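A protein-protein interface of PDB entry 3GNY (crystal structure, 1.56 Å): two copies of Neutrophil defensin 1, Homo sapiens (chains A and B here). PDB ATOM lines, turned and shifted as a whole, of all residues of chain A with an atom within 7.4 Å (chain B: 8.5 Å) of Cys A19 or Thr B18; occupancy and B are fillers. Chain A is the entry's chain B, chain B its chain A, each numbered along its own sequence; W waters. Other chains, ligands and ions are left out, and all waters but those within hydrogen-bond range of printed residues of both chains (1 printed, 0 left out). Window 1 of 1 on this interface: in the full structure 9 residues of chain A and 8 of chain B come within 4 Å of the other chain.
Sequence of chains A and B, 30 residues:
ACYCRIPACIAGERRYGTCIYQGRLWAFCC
The backbone NH of Ile A20 lies within hydrogen-bond range of the backbone carbonyl oxygen of Thr B18, at 2.7 Å. The backbone carbonyl oxygen of Thr A18 is in hydrogen-bond range of the backbone NH of Ile B20, 2.8 Å away.
SG of Cys B19 is disulfide-bonded to SG of Cys B4. NE of Arg B15 lies within hydrogen-bond range of O of Gly B17 (2.9 Å). The backbone NH of Tyr B16 is in hydrogen-bond range of the backbone carbonyl oxygen of Phe B28 (2.8 Å). The backbone carbonyl oxygen (O) of Gly A17 sits at hydrogen-bond distance from the guanidinium group (NE) of Arg A15, at 3.0 Å. N of Phe A28 is in hydrogen-bond range of O of Gly A17 (2.9 Å). The backbone NH (N) of Cys A19 lies within hydrogen-bond range of the backbone carbonyl oxygen (O) of Trp A26 (2.8 Å).
Among the printed residues, merely in contact across the chains: Ile A20 with Gly B17 (3.1 Å), Gly A17 with Ile B20 (3.1 Å), Tyr A21 with Tyr B16 (3.3 Å), Tyr A21 with Phe B28 (3.4 Å), Thr A18 with Cys B19 (3.4 Å), Phe A28 with Tyr B21 (3.4 Å), Phe A28 with Cys B4 (3.5 Å), Cys A19 with Thr B18 (3.6 Å), Cys A4 with Phe B28 (3.7 Å) and Gln A22 with Tyr B16 (3.9 Å).
Printed residues of chain B within 4 Å of Cys A19: Thr B18 (3.6 Å). Printed residues of chain A within 4 Å of Tyr B16: Tyr A21 (3.3 Å) and Gln A22 (3.9 Å). Thr B18 touches just these residues of chain A: Cys A19 (3.6 Å) and Ile A20 (2.7 Å). Printed residues of chain A within 4 Å of Phe B28: Cys A4 (3.7 Å) and Tyr A21 (3.4 Å). The nearest residue of chain B that does not touch Cys A19 is Cys B19 (4.3 Å). The nearest residue of chain A that does not touch Thr B18 is Thr A18 (4.2 Å).
Of the 17 printed residues of chain B, 8 touch a printed residue of chain A. Printed residues of chain A that touch a printed residue of chain B: Cys A4, Gly A17, Thr A18, Cys A19, Ile A20, Tyr A21, Gln A22 and Phe A28. Hydrophobic or aromatic side chains of chain A that line the printed part of chain B: Ile A20, Tyr A21 and Phe A28.
Cys A4 touches Phe B28, and with the chains exchanged Phe A28 touches Cys B4. Gly A17 touches Ile B20, and with the chains exchanged Ile A20 touches Gly B17. Thr A18 touches Cys B19, and with the chains exchanged Cys A19 touches Thr B18. Tyr A21 touches Phe B28, and with the chains exchanged Phe A28 touches Tyr B21. Positions printed for both chains: 3, 4, 5, 15, 17, 18, 19, 20, 21, 24, 25, 26, 27, 28 and 29.
Water W1 lies within hydrogen-bond range of OE1 of Gln A22 (2.6 Å) and O of Tyr B16 (2.7 Å).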
ATOM      1  N   TYR A   3     -29.005  22.239   5.662  1.00  0.00           N
ATOM      2  CA  TYR A   3     -27.764  21.871   6.331  1.00  0.00           C
ATOM      3  C   TYR A   3     -27.028  20.787   5.577  1.00  0.00           C
ATOM      4  O   TYR A   3     -27.643  19.825   5.101  1.00  0.00           O
ATOM      5  CB  TYR A   3     -28.064  21.349   7.738  1.00  0.00           C
ATOM      6  CG  TYR A   3     -28.667  22.410   8.618  1.00  0.00           C
ATOM      7  CD1 TYR A   3     -27.854  23.352   9.241  1.00  0.00           C
ATOM      8  CD2 TYR A   3     -30.041  22.517   8.765  1.00  0.00           C
ATOM      9  CE1 TYR A   3     -28.391  24.366  10.040  1.00  0.00           C
ATOM     10  CE2 TYR A   3     -30.603  23.537   9.571  1.00  0.00           C
ATOM     11  CZ  TYR A   3     -29.761  24.454  10.197  1.00  0.00           C
ATOM     12  OH  TYR A   3     -30.279  25.463  10.988  1.00  0.00           O
ATOM     13  N   CYS A   4     -25.707  20.949   5.468  1.00  0.00           N
ATOM     14  CA  CYS A   4     -24.818  19.876   5.003  1.00  0.00           C
ATOM     15  C   CYS A   4     -24.529  18.923   6.159  1.00  0.00           C
ATOM     16  O   CYS A   4     -24.029  19.364   7.202  1.00  0.00           O
ATOM     17  CB  CYS A   4     -23.511  20.443   4.440  1.00  0.00           C
ATOM     18  SG  CYS A   4     -23.729  21.585   3.059  1.00  0.00           S
ATOM     19  N   ARG A   5     -24.835  17.635   5.992  1.00  0.00           N
ATOM     20  CA  ARG A   5     -24.701  16.662   7.090  1.00  0.00           C
ATOM     21  C   ARG A   5     -23.933  15.388   6.725  1.00  0.00           C
ATOM     22  O   ARG A   5     -24.035  14.890   5.610  1.00  0.00           O
ATOM     23  CB  ARG A   5     -26.079  16.241   7.619  1.00  0.00           C
ATOM     24  CG  ARG A   5     -27.009  17.368   8.025  1.00  0.00           C
ATOM     25  CD  ARG A   5     -28.080  16.835   8.952  1.00  0.00           C
ATOM     26  NE  ARG A   5     -29.073  17.850   9.294  1.00  0.00           N
ATOM     27  CZ  ARG A   5     -28.963  18.709  10.311  1.00  0.00           C
ATOM     28  NH1 ARG A   5     -27.888  18.711  11.087  1.00  0.00           N
ATOM     29  NH2 ARG A   5     -29.928  19.583  10.535  1.00  0.00           N
ATOM     30  N   ARG A  15     -33.111  14.641   1.873  1.00  0.00           N
ATOM     31  CA  ARG A  15     -31.873  14.956   1.163  1.00  0.00           C
ATOM     32  C   ARG A  15     -32.238  15.504  -0.207  1.00  0.00           C
ATOM     33  O   ARG A  15     -32.873  14.822  -1.026  1.00  0.00           O
ATOM     34  CB  ARG A  15     -30.972  13.731   1.003  1.00  0.00           C
ATOM     35  CG  ARG A  15     -29.669  14.114   0.391  1.00  0.00           C
ATOM     36  CD  ARG A  15     -28.737  12.957   0.261  1.00  0.00           C
ATOM     37  NE  ARG A  15     -27.514  13.367  -0.420  1.00  0.00           N
ATOM     38  CZ  ARG A  15     -26.357  12.726  -0.314  1.00  0.00           C
ATOM     39  NH1 ARG A  15     -26.274  11.653   0.468  1.00  0.00           N
ATOM     40  NH2 ARG A  15     -25.275  13.164  -0.967  1.00  0.00           N
ATOM     41  N   GLY A  17     -29.746  17.289  -2.052  1.00  0.00           N
ATOM     42  CA  GLY A  17     -28.555  17.494  -2.819  1.00  0.00           C
ATOM     43  C   GLY A  17     -27.332  17.067  -2.074  1.00  0.00           C
ATOM     44  O   GLY A  17     -27.405  16.249  -1.169  1.00  0.00           O
ATOM     45  N   THR A  18     -26.197  17.634  -2.480  1.00  0.00           N
ATOM     46  CA  THR A  18     -24.873  17.237  -1.979  1.00  0.00           C
ATOM     47  C   THR A  18     -24.000  18.467  -1.771  1.00  0.00           C
ATOM     48  O   THR A  18     -24.031  19.379  -2.587  1.00  0.00           O
ATOM     49  CB  THR A  18     -24.198  16.296  -2.993  1.00  0.00           C
ATOM     50  OG1 THR A  18     -25.045  15.164  -3.191  1.00  0.00           O
ATOM     51  CG2 THR A  18     -22.811  15.841  -2.505  1.00  0.00           C
ATOM     52  N   CYS A  19     -23.235  18.486  -0.682  1.00  0.00           N
ATOM     53  CA  CYS A  19     -22.215  19.529  -0.490  1.00  0.00           C
ATOM     54  C   CYS A  19     -20.843  18.908  -0.689  1.00  0.00           C
ATOM     55  O   CYS A  19     -20.604  17.749  -0.307  1.00  0.00           O
ATOM     56  CB  CYS A  19     -22.271  20.106   0.914  1.00  0.00           C
ATOM     57  SG  CYS A  19     -23.967  20.380   1.446  1.00  0.00           S
ATOM     58  N   ILE A  20     -19.953  19.671  -1.298  1.00  0.00           N
ATOM     59  CA  ILE A  20     -18.560  19.268  -1.437  1.00  0.00           C
ATOM     60  C   ILE A  20     -17.708  20.317  -0.757  1.00  0.00           C
ATOM     61  O   ILE A  20     -17.675  21.466  -1.192  1.00  0.00           O
ATOM     62  CB  ILE A  20     -18.129  19.196  -2.916  1.00  0.00           C
ATOM     63  CG1 ILE A  20     -19.018  18.230  -3.686  1.00  0.00           C
ATOM     64  CG2 ILE A  20     -16.649  18.770  -3.021  1.00  0.00           C
ATOM     65  CD1 ILE A  20     -18.687  18.248  -5.148  1.00  0.00           C
ATOM     66  N   TYR A  21     -17.039  19.929   0.319  1.00  0.00           N
ATOM     67  CA  TYR A  21     -16.070  20.831   0.933  1.00  0.00           C
ATOM     68  C   TYR A  21     -15.086  20.137   1.818  1.00  0.00           C
ATOM     69  O   TYR A  21     -15.362  19.059   2.334  1.00  0.00           O
ATOM     70  CB  TYR A  21     -16.739  22.018   1.643  1.00  0.00           C
ATOM     71  CG  TYR A  21     -17.666  21.684   2.786  1.00  0.00           C
ATOM     72  CD1 TYR A  21     -19.008  21.399   2.556  1.00  0.00           C
ATOM     73  CD2 TYR A  21     -17.205  21.700   4.102  1.00  0.00           C
ATOM     74  CE1 TYR A  21     -19.879  21.103   3.618  1.00  0.00           C
ATOM     75  CE2 TYR A  21     -18.062  21.405   5.176  1.00  0.00           C
ATOM     76  CZ  TYR A  21     -19.398  21.114   4.924  1.00  0.00           C
ATOM     77  OH  TYR A  21     -20.239  20.841   5.986  1.00  0.00           O
ATOM     78  N   GLN A  22     -13.918  20.759   1.961  1.00  0.00           N
ATOM     79  CA  GLN A  22     -12.825  20.197   2.745  1.00  0.00           C
ATOM     80  C   GLN A  22     -12.498  18.773   2.222  1.00  0.00           C
ATOM     81  O   GLN A  22     -12.148  17.899   2.997  1.00  0.00           O
ATOM     82  CB  GLN A  22     -13.204  20.198   4.253  1.00  0.00           C
ATOM     83  CG  GLN A  22     -13.549  21.589   4.881  1.00  0.00           C
ATOM     84  CD  GLN A  22     -12.345  22.524   4.934  1.00  0.00           C
ATOM     85  OE1 GLN A  22     -11.925  23.080   3.909  1.00  0.00           O
ATOM     86  NE2 GLN A  22     -11.774  22.689   6.118  1.00  0.00           N
ATOM     87  N   ARG A  24     -14.548  16.500   1.063  1.00  0.00           N
ATOM     88  CA  ARG A  24     -15.510  15.532   1.589  1.00  0.00           C
ATOM     89  C   ARG A  24     -16.880  15.774   0.998  1.00  0.00           C
ATOM     90  O   ARG A  24     -17.217  16.901   0.624  1.00  0.00           O
ATOM     91  CB  ARG A  24     -15.600  15.627   3.129  1.00  0.00           C
ATOM     92  CG  ARG A  24     -14.251  15.424   3.788  1.00  0.00           C
ATOM     93  CD  ARG A  24     -14.202  15.951   5.212  1.00  0.00           C
ATOM     94  NE  ARG A  24     -15.156  15.247   6.045  1.00  0.00           N
ATOM     95  CZ  ARG A  24     -15.467  15.604   7.290  1.00  0.00           C
ATOM     96  NH1 ARG A  24     -16.333  14.882   7.975  1.00  0.00           N
ATOM     97  NH2 ARG A  24     -14.918  16.676   7.860  1.00  0.00           N
ATOM     98  N   LEU A  25     -17.668  14.701   0.973  1.00  0.00           N
ATOM     99  CA  LEU A  25     -19.050  14.710   0.500  1.00  0.00           C
ATOM    100  C   LEU A  25     -20.014  14.721   1.673  1.00  0.00           C
ATOM    101  O   LEU A  25     -19.834  13.953   2.628  1.00  0.00           O
ATOM    102  CB  LEU A  25     -19.319  13.483  -0.365  1.00  0.00           C
ATOM    103  CG  LEU A  25     -18.617  13.487  -1.733  1.00  0.00           C
ATOM    104  CD1 LEU A  25     -18.486  12.090  -2.309  1.00  0.00           C
ATOM    105  CD2 LEU A  25     -19.373  14.393  -2.701  1.00  0.00           C
ATOM    106  N   TRP A  26     -21.031  15.587   1.603  1.00  0.00           N
ATOM    107  CA  TRP A  26     -22.029  15.764   2.653  1.00  0.00           C
ATOM    108  C   TRP A  26     -23.417  15.702   2.025  1.00  0.00           C
ATOM    109  O   TRP A  26     -23.604  16.131   0.879  1.00  0.00           O
ATOM    110  CB  TRP A  26     -21.874  17.130   3.320  1.00  0.00           C
ATOM    111  CG  TRP A  26     -20.492  17.461   3.750  1.00  0.00           C
ATOM    112  CD1 TRP A  26     -19.431  17.766   2.928  1.00  0.00           C
ATOM    113  CD2 TRP A  26     -20.015  17.598   5.085  1.00  0.00           C
ATOM    114  NE1 TRP A  26     -18.314  18.036   3.682  1.00  0.00           N
ATOM    115  CE2 TRP A  26     -18.637  17.923   5.008  1.00  0.00           C
ATOM    116  CE3 TRP A  26     -20.595  17.417   6.342  1.00  0.00           C
ATOM    117  CZ2 TRP A  26     -17.847  18.124   6.139  1.00  0.00           C
ATOM    118  CZ3 TRP A  26     -19.805  17.600   7.466  1.00  0.00           C
ATOM    119  CH2 TRP A  26     -18.439  17.943   7.358  1.00  0.00           C
ATOM    120  N   ALA A  27     -24.398  15.174   2.759  1.00  0.00           N
ATOM    121  CA  ALA A  27     -25.793  15.250   2.311  1.00  0.00           C
ATOM    122  C   ALA A  27     -26.302  16.683   2.527  1.00  0.00           C
ATOM    123  O   ALA A  27     -26.029  17.298   3.561  1.00  0.00           O
ATOM    124  CB  ALA A  27     -26.663  14.245   3.063  1.00  0.00           C
ATOM    125  N   PHE A  28     -27.031  17.214   1.550  1.00  0.00           N
ATOM    126  CA  PHE A  28     -27.652  18.525   1.712  1.00  0.00           C
ATOM    127  C   PHE A  28     -29.111  18.298   2.074  1.00  0.00           C
ATOM    128  O   PHE A  28     -29.879  17.750   1.272  1.00  0.00           O
ATOM    129  CB  PHE A  28     -27.490  19.393   0.450  1.00  0.00           C
ATOM    130  CG  PHE A  28     -27.877  20.846   0.645  1.00  0.00           C
ATOM    131  CD1 PHE A  28     -27.206  21.665   1.564  1.00  0.00           C
ATOM    132  CD2 PHE A  28     -28.907  21.411  -0.090  1.00  0.00           C
ATOM    133  CE1 PHE A  28     -27.560  23.015   1.722  1.00  0.00           C
ATOM    134  CE2 PHE A  28     -29.276  22.761   0.068  1.00  0.00           C
ATOM    135  CZ  PHE A  28     -28.590  23.554   0.972  1.00  0.00           C
ATOM    136  N   CYS A  29     -29.459  18.693   3.295  1.00  0.00           N
ATOM    137  CA  CYS A  29     -30.704  18.289   3.954  1.00  0.00           C
ATOM    138  C   CYS A  29     -31.580  19.484   4.247  1.00  0.00           C
ATOM    139  O   CYS A  29     -31.089  20.480   4.759  1.00  0.00           O
ATOM    140  CB  CYS A  29     -30.351  17.634   5.301  1.00  0.00           C
ATOM    141  SG  CYS A  29     -29.236  16.224   5.151  1.00  0.00           S
ATOM    142  N   CYS B   2     -22.625  28.348   7.836  1.00  0.00           N
ATOM    143  CA  CYS B   2     -22.292  28.277   6.419  1.00  0.00           C
ATOM    144  C   CYS B   2     -23.549  28.302   5.576  1.00  0.00           C
ATOM    145  O   CYS B   2     -24.620  27.887   6.018  1.00  0.00           O
ATOM    146  CB  CYS B   2     -21.480  27.010   6.095  1.00  0.00           C
ATOM    147  SG  CYS B   2     -19.903  26.817   6.999  1.00  0.00           S
ATOM    148  N   TYR B   3     -23.388  28.759   4.335  1.00  0.00           N
ATOM    149  CA  TYR B   3     -24.496  28.923   3.419  1.00  0.00           C
ATOM    150  C   TYR B   3     -24.130  28.482   2.017  1.00  0.00           C
ATOM    151  O   TYR B   3     -23.041  28.811   1.523  1.00  0.00           O
ATOM    152  CB  TYR B   3     -24.892  30.407   3.348  1.00  0.00           C
ATOM    153  CG  TYR B   3     -25.315  30.965   4.676  1.00  0.00           C
ATOM    154  CD1 TYR B   3     -26.616  30.801   5.124  1.00  0.00           C
ATOM    155  CD2 TYR B   3     -24.405  31.624   5.498  1.00  0.00           C
ATOM    156  CE1 TYR B   3     -27.013  31.302   6.363  1.00  0.00           C
ATOM    157  CE2 TYR B   3     -24.782  32.126   6.732  1.00  0.00           C
ATOM    158  CZ  TYR B   3     -26.084  31.963   7.156  1.00  0.00           C
ATOM    159  OH  TYR B   3     -26.483  32.453   8.375  1.00  0.00           O
ATOM    160  N   CYS B   4     -25.054  27.789   1.359  1.00  0.00           N
ATOM    161  CA  CYS B   4     -24.963  27.617  -0.099  1.00  0.00           C
ATOM    162  C   CYS B   4     -25.558  28.856  -0.767  1.00  0.00           C
ATOM    163  O   CYS B   4     -26.714  29.239  -0.472  1.00  0.00           O
ATOM    164  CB  CYS B   4     -25.736  26.364  -0.552  1.00  0.00           C
ATOM    165  SG  CYS B   4     -25.080  24.830   0.112  1.00  0.00           S
ATOM    166  N   ARG B   5     -24.774  29.493  -1.645  1.00  0.00           N
ATOM    167  CA  ARG B   5     -25.165  30.773  -2.258  1.00  0.00           C
ATOM    168  C   ARG B   5     -25.051  30.795  -3.769  1.00  0.00           C
ATOM    169  O   ARG B   5     -24.125  30.221  -4.334  1.00  0.00           O
ATOM    170  CB  ARG B   5     -24.327  31.924  -1.692  1.00  0.00           C
ATOM    171  CG  ARG B   5     -24.492  32.165  -0.187  1.00  0.00           C
ATOM    172  CD  ARG B   5     -23.905  33.522   0.122  1.00  0.00           C
ATOM    173  NE  ARG B   5     -23.864  33.804   1.547  1.00  0.00           N
ATOM    174  CZ  ARG B   5     -24.930  34.153   2.275  1.00  0.00           C
ATOM    175  NH1 ARG B   5     -26.136  34.258   1.707  1.00  0.00           N
ATOM    176  NH2 ARG B   5     -24.800  34.388   3.582  1.00  0.00           N
ATOM    177  N   ARG B  15     -15.236  31.140   0.319  1.00  0.00           N
ATOM    178  CA  ARG B  15     -15.736  29.953  -0.349  1.00  0.00           C
ATOM    179  C   ARG B  15     -14.903  28.734   0.050  1.00  0.00           C
ATOM    180  O   ARG B  15     -13.681  28.703  -0.133  1.00  0.00           O
ATOM    181  CB  ARG B  15     -15.758  30.107  -1.879  1.00  0.00           C
ATOM    182  CG  ARG B  15     -16.343  28.871  -2.558  1.00  0.00           C
ATOM    183  CD  ARG B  15     -16.624  29.102  -4.029  1.00  0.00           C
ATOM    184  NE  ARG B  15     -17.247  27.935  -4.637  1.00  0.00           N
ATOM    185  CZ  ARG B  15     -17.860  27.924  -5.816  1.00  0.00           C
ATOM    186  NH1 ARG B  15     -17.967  29.043  -6.531  1.00  0.00           N
ATOM    187  NH2 ARG B  15     -18.379  26.792  -6.283  1.00  0.00           N
ATOM    188  N   TYR B  16     -15.573  27.731   0.610  1.00  0.00           N
ATOM    189  CA  TYR B  16     -14.916  26.497   1.022  1.00  0.00           C
ATOM    190  C   TYR B  16     -15.292  25.293   0.163  1.00  0.00           C
ATOM    191  O   TYR B  16     -14.717  24.223   0.332  1.00  0.00           O
ATOM    192  CB  TYR B  16     -15.212  26.167   2.489  1.00  0.00           C
ATOM    193  CG  TYR B  16     -14.548  27.080   3.483  1.00  0.00           C
ATOM    194  CD1 TYR B  16     -13.347  26.742   4.056  1.00  0.00           C
ATOM    195  CD2 TYR B  16     -15.162  28.258   3.864  1.00  0.00           C
ATOM    196  CE1 TYR B  16     -12.753  27.568   4.984  1.00  0.00           C
ATOM    197  CE2 TYR B  16     -14.588  29.102   4.786  1.00  0.00           C
ATOM    198  CZ  TYR B  16     -13.382  28.752   5.341  1.00  0.00           C
ATOM    199  OH  TYR B  16     -12.795  29.585   6.264  1.00  0.00           O
ATOM    200  N   GLY B  17     -16.257  25.447  -0.750  1.00  0.00           N
ATOM    201  CA  GLY B  17     -16.647  24.342  -1.626  1.00  0.00           C
ATOM    202  C   GLY B  17     -17.847  24.698  -2.462  1.00  0.00           C
ATOM    203  O   GLY B  17     -18.075  25.858  -2.794  1.00  0.00           O
ATOM    204  N   THR B  18     -18.614  23.666  -2.795  1.00  0.00           N
ATOM    205  CA  THR B  18     -19.696  23.757  -3.755  1.00  0.00           C
ATOM    206  C   THR B  18     -20.881  22.951  -3.276  1.00  0.00           C
ATOM    207  O   THR B  18     -20.705  21.903  -2.668  1.00  0.00           O
ATOM    208  CB  THR B  18     -19.246  23.188  -5.118  1.00  0.00           C
ATOM    209  OG1 THR B  18     -18.131  23.966  -5.579  1.00  0.00           O
ATOM    210  CG2 THR B  18     -20.367  23.248  -6.164  1.00  0.00           C
ATOM    211  N   CYS B  19     -22.085  23.453  -3.513  1.00  0.00           N
ATOM    212  CA  CYS B  19     -23.306  22.668  -3.269  1.00  0.00           C
ATOM    213  C   CYS B  19     -23.972  22.338  -4.587  1.00  0.00           C
ATOM    214  O   CYS B  19     -23.939  23.138  -5.543  1.00  0.00           O
ATOM    215  CB  CYS B  19     -24.320  23.412  -2.404  1.00  0.00           C
ATOM    216  SG  CYS B  19     -23.536  24.371  -1.098  1.00  0.00           S
ATOM    217  N   ILE B  20     -24.613  21.180  -4.619  1.00  0.00           N
ATOM    218  CA  ILE B  20     -25.425  20.726  -5.743  1.00  0.00           C
ATOM    219  C   ILE B  20     -26.846  20.613  -5.182  1.00  0.00           C
ATOM    220  O   ILE B  20     -27.099  19.841  -4.257  1.00  0.00           O
ATOM    221  CB  ILE B  20     -24.975  19.334  -6.238  1.00  0.00           C
ATOM    222  CG1 ILE B  20     -23.544  19.380  -6.766  1.00  0.00           C
ATOM    223  CG2 ILE B  20     -25.961  18.788  -7.294  1.00  0.00           C
ATOM    224  CD1 ILE B  20     -22.933  17.985  -6.998  1.00  0.00           C
ATOM    225  N   TYR B  21     -27.767  21.424  -5.718  1.00  0.00           N
ATOM    226  CA  TYR B  21     -29.106  21.548  -5.149  1.00  0.00           C
ATOM    227  C   TYR B  21     -30.007  22.228  -6.186  1.00  0.00           C
ATOM    228  O   TYR B  21     -29.615  23.209  -6.840  1.00  0.00           O
ATOM    229  CB  TYR B  21     -29.021  22.345  -3.845  1.00  0.00           C
ATOM    230  CG  TYR B  21     -30.334  22.768  -3.208  1.00  0.00           C
ATOM    231  CD1 TYR B  21     -31.243  21.824  -2.722  1.00  0.00           C
ATOM    232  CD2 TYR B  21     -30.651  24.127  -3.065  1.00  0.00           C
ATOM    233  CE1 TYR B  21     -32.453  22.230  -2.107  1.00  0.00           C
ATOM    234  CE2 TYR B  21     -31.848  24.536  -2.472  1.00  0.00           C
ATOM    235  CZ  TYR B  21     -32.740  23.593  -1.995  1.00  0.00           C
ATOM    236  OH  TYR B  21     -33.915  24.000  -1.417  1.00  0.00           O
ATOM    237  N   ARG B  24     -28.798  23.155  -9.710  1.00  0.00           N
ATOM    238  CA  ARG B  24     -27.803  24.213  -9.808  1.00  0.00           C
ATOM    239  C   ARG B  24     -26.573  23.991  -8.923  1.00  0.00           C
ATOM    240  O   ARG B  24     -26.606  23.222  -7.924  1.00  0.00           O
ATOM    241  CB  ARG B  24     -28.440  25.538  -9.410  1.00  0.00           C
ATOM    242  CG  ARG B  24     -29.565  25.980 -10.354  1.00  0.00           C
ATOM    243  CD  ARG B  24     -29.045  26.429 -11.746  1.00  0.00           C
ATOM    244  NE  ARG B  24     -28.122  27.554 -11.589  1.00  0.00           N
ATOM    245  CZ  ARG B  24     -28.511  28.817 -11.385  1.00  0.00           C
ATOM    246  NH1 ARG B  24     -29.813  29.127 -11.392  1.00  0.00           N
ATOM    247  NH2 ARG B  24     -27.603  29.773 -11.227  1.00  0.00           N
ATOM    248  N   LEU B  25     -25.488  24.644  -9.341  1.00  0.00           N
ATOM    249  CA  LEU B  25     -24.280  24.774  -8.545  1.00  0.00           C
ATOM    250  C   LEU B  25     -24.335  26.027  -7.676  1.00  0.00           C
ATOM    251  O   LEU B  25     -24.724  27.124  -8.138  1.00  0.00           O
ATOM    252  CB  LEU B  25     -23.059  24.846  -9.471  1.00  0.00           C
ATOM    253  CG  LEU B  25     -22.792  23.532 -10.223  1.00  0.00           C
ATOM    254  CD1 LEU B  25     -21.870  23.729 -11.402  1.00  0.00           C
ATOM    255  CD2 LEU B  25     -22.203  22.505  -9.294  1.00  0.00           C
ATOM    256  N   TRP B  26     -23.907  25.851  -6.424  1.00  0.00           N
ATOM    257  CA  TRP B  26     -23.887  26.919  -5.423  1.00  0.00           C
ATOM    258  C   TRP B  26     -22.499  27.023  -4.800  1.00  0.00           C
ATOM    259  O   TRP B  26     -21.809  26.029  -4.649  1.00  0.00           O
ATOM    260  CB  TRP B  26     -24.881  26.617  -4.290  1.00  0.00           C
ATOM    261  CG  TRP B  26     -26.284  26.317  -4.712  1.00  0.00           C
ATOM    262  CD1 TRP B  26     -26.706  25.274  -5.489  1.00  0.00           C
ATOM    263  CD2 TRP B  26     -27.444  27.088  -4.400  1.00  0.00           C
ATOM    264  NE1 TRP B  26     -28.072  25.335  -5.668  1.00  0.00           N
ATOM    265  CE2 TRP B  26     -28.553  26.453  -5.026  1.00  0.00           C
ATOM    266  CE3 TRP B  26     -27.663  28.257  -3.636  1.00  0.00           C
ATOM    267  CZ2 TRP B  26     -29.859  26.931  -4.895  1.00  0.00           C
ATOM    268  CZ3 TRP B  26     -28.960  28.736  -3.511  1.00  0.00           C
ATOM    269  CH2 TRP B  26     -30.048  28.081  -4.151  1.00  0.00           C
ATOM    270  N   ALA B  27     -22.087  28.235  -4.432  1.00  0.00           N
ATOM    271  CA  ALA B  27     -20.882  28.379  -3.628  1.00  0.00           C
ATOM    272  C   ALA B  27     -21.207  27.985  -2.202  1.00  0.00           C
ATOM    273  O   ALA B  27     -22.205  28.428  -1.655  1.00  0.00           O
ATOM    274  CB  ALA B  27     -20.379  29.800  -3.681  1.00  0.00           C
ATOM    275  N   PHE B  28     -20.356  27.165  -1.592  1.00  0.00           N
ATOM    276  CA  PHE B  28     -20.459  26.902  -0.162  1.00  0.00           C
ATOM    277  C   PHE B  28     -19.578  27.876   0.622  1.00  0.00           C
ATOM    278  O   PHE B  28     -18.345  27.867   0.474  1.00  0.00           O
ATOM    279  CB  PHE B  28     -20.083  25.457   0.140  1.00  0.00           C
ATOM    280  CG  PHE B  28     -20.209  25.091   1.589  1.00  0.00           C
ATOM    281  CD1 PHE B  28     -21.464  24.913   2.170  1.00  0.00           C
ATOM    282  CD2 PHE B  28     -19.077  24.936   2.374  1.00  0.00           C
ATOM    283  CE1 PHE B  28     -21.568  24.574   3.514  1.00  0.00           C
ATOM    284  CE2 PHE B  28     -19.183  24.607   3.706  1.00  0.00           C
ATOM    285  CZ  PHE B  28     -20.429  24.429   4.264  1.00  0.00           C
ATOM    286  N   CYS B  29     -20.240  28.715   1.433  1.00  0.00           N
ATOM    287  CA  CYS B  29     -19.625  29.899   2.025  1.00  0.00           C
ATOM    288  C   CYS B  29     -19.692  29.877   3.530  1.00  0.00           C
ATOM    289  O   CYS B  29     -20.734  29.583   4.085  1.00  0.00           O
ATOM    290  CB  CYS B  29     -20.399  31.117   1.534  1.00  0.00           C
ATOM    291  SG  CYS B  29     -20.531  31.230  -0.275  1.00  0.00           S
HETATM  292  O   HOH W   1     -12.359  23.284   1.305  1.00  0.00           O
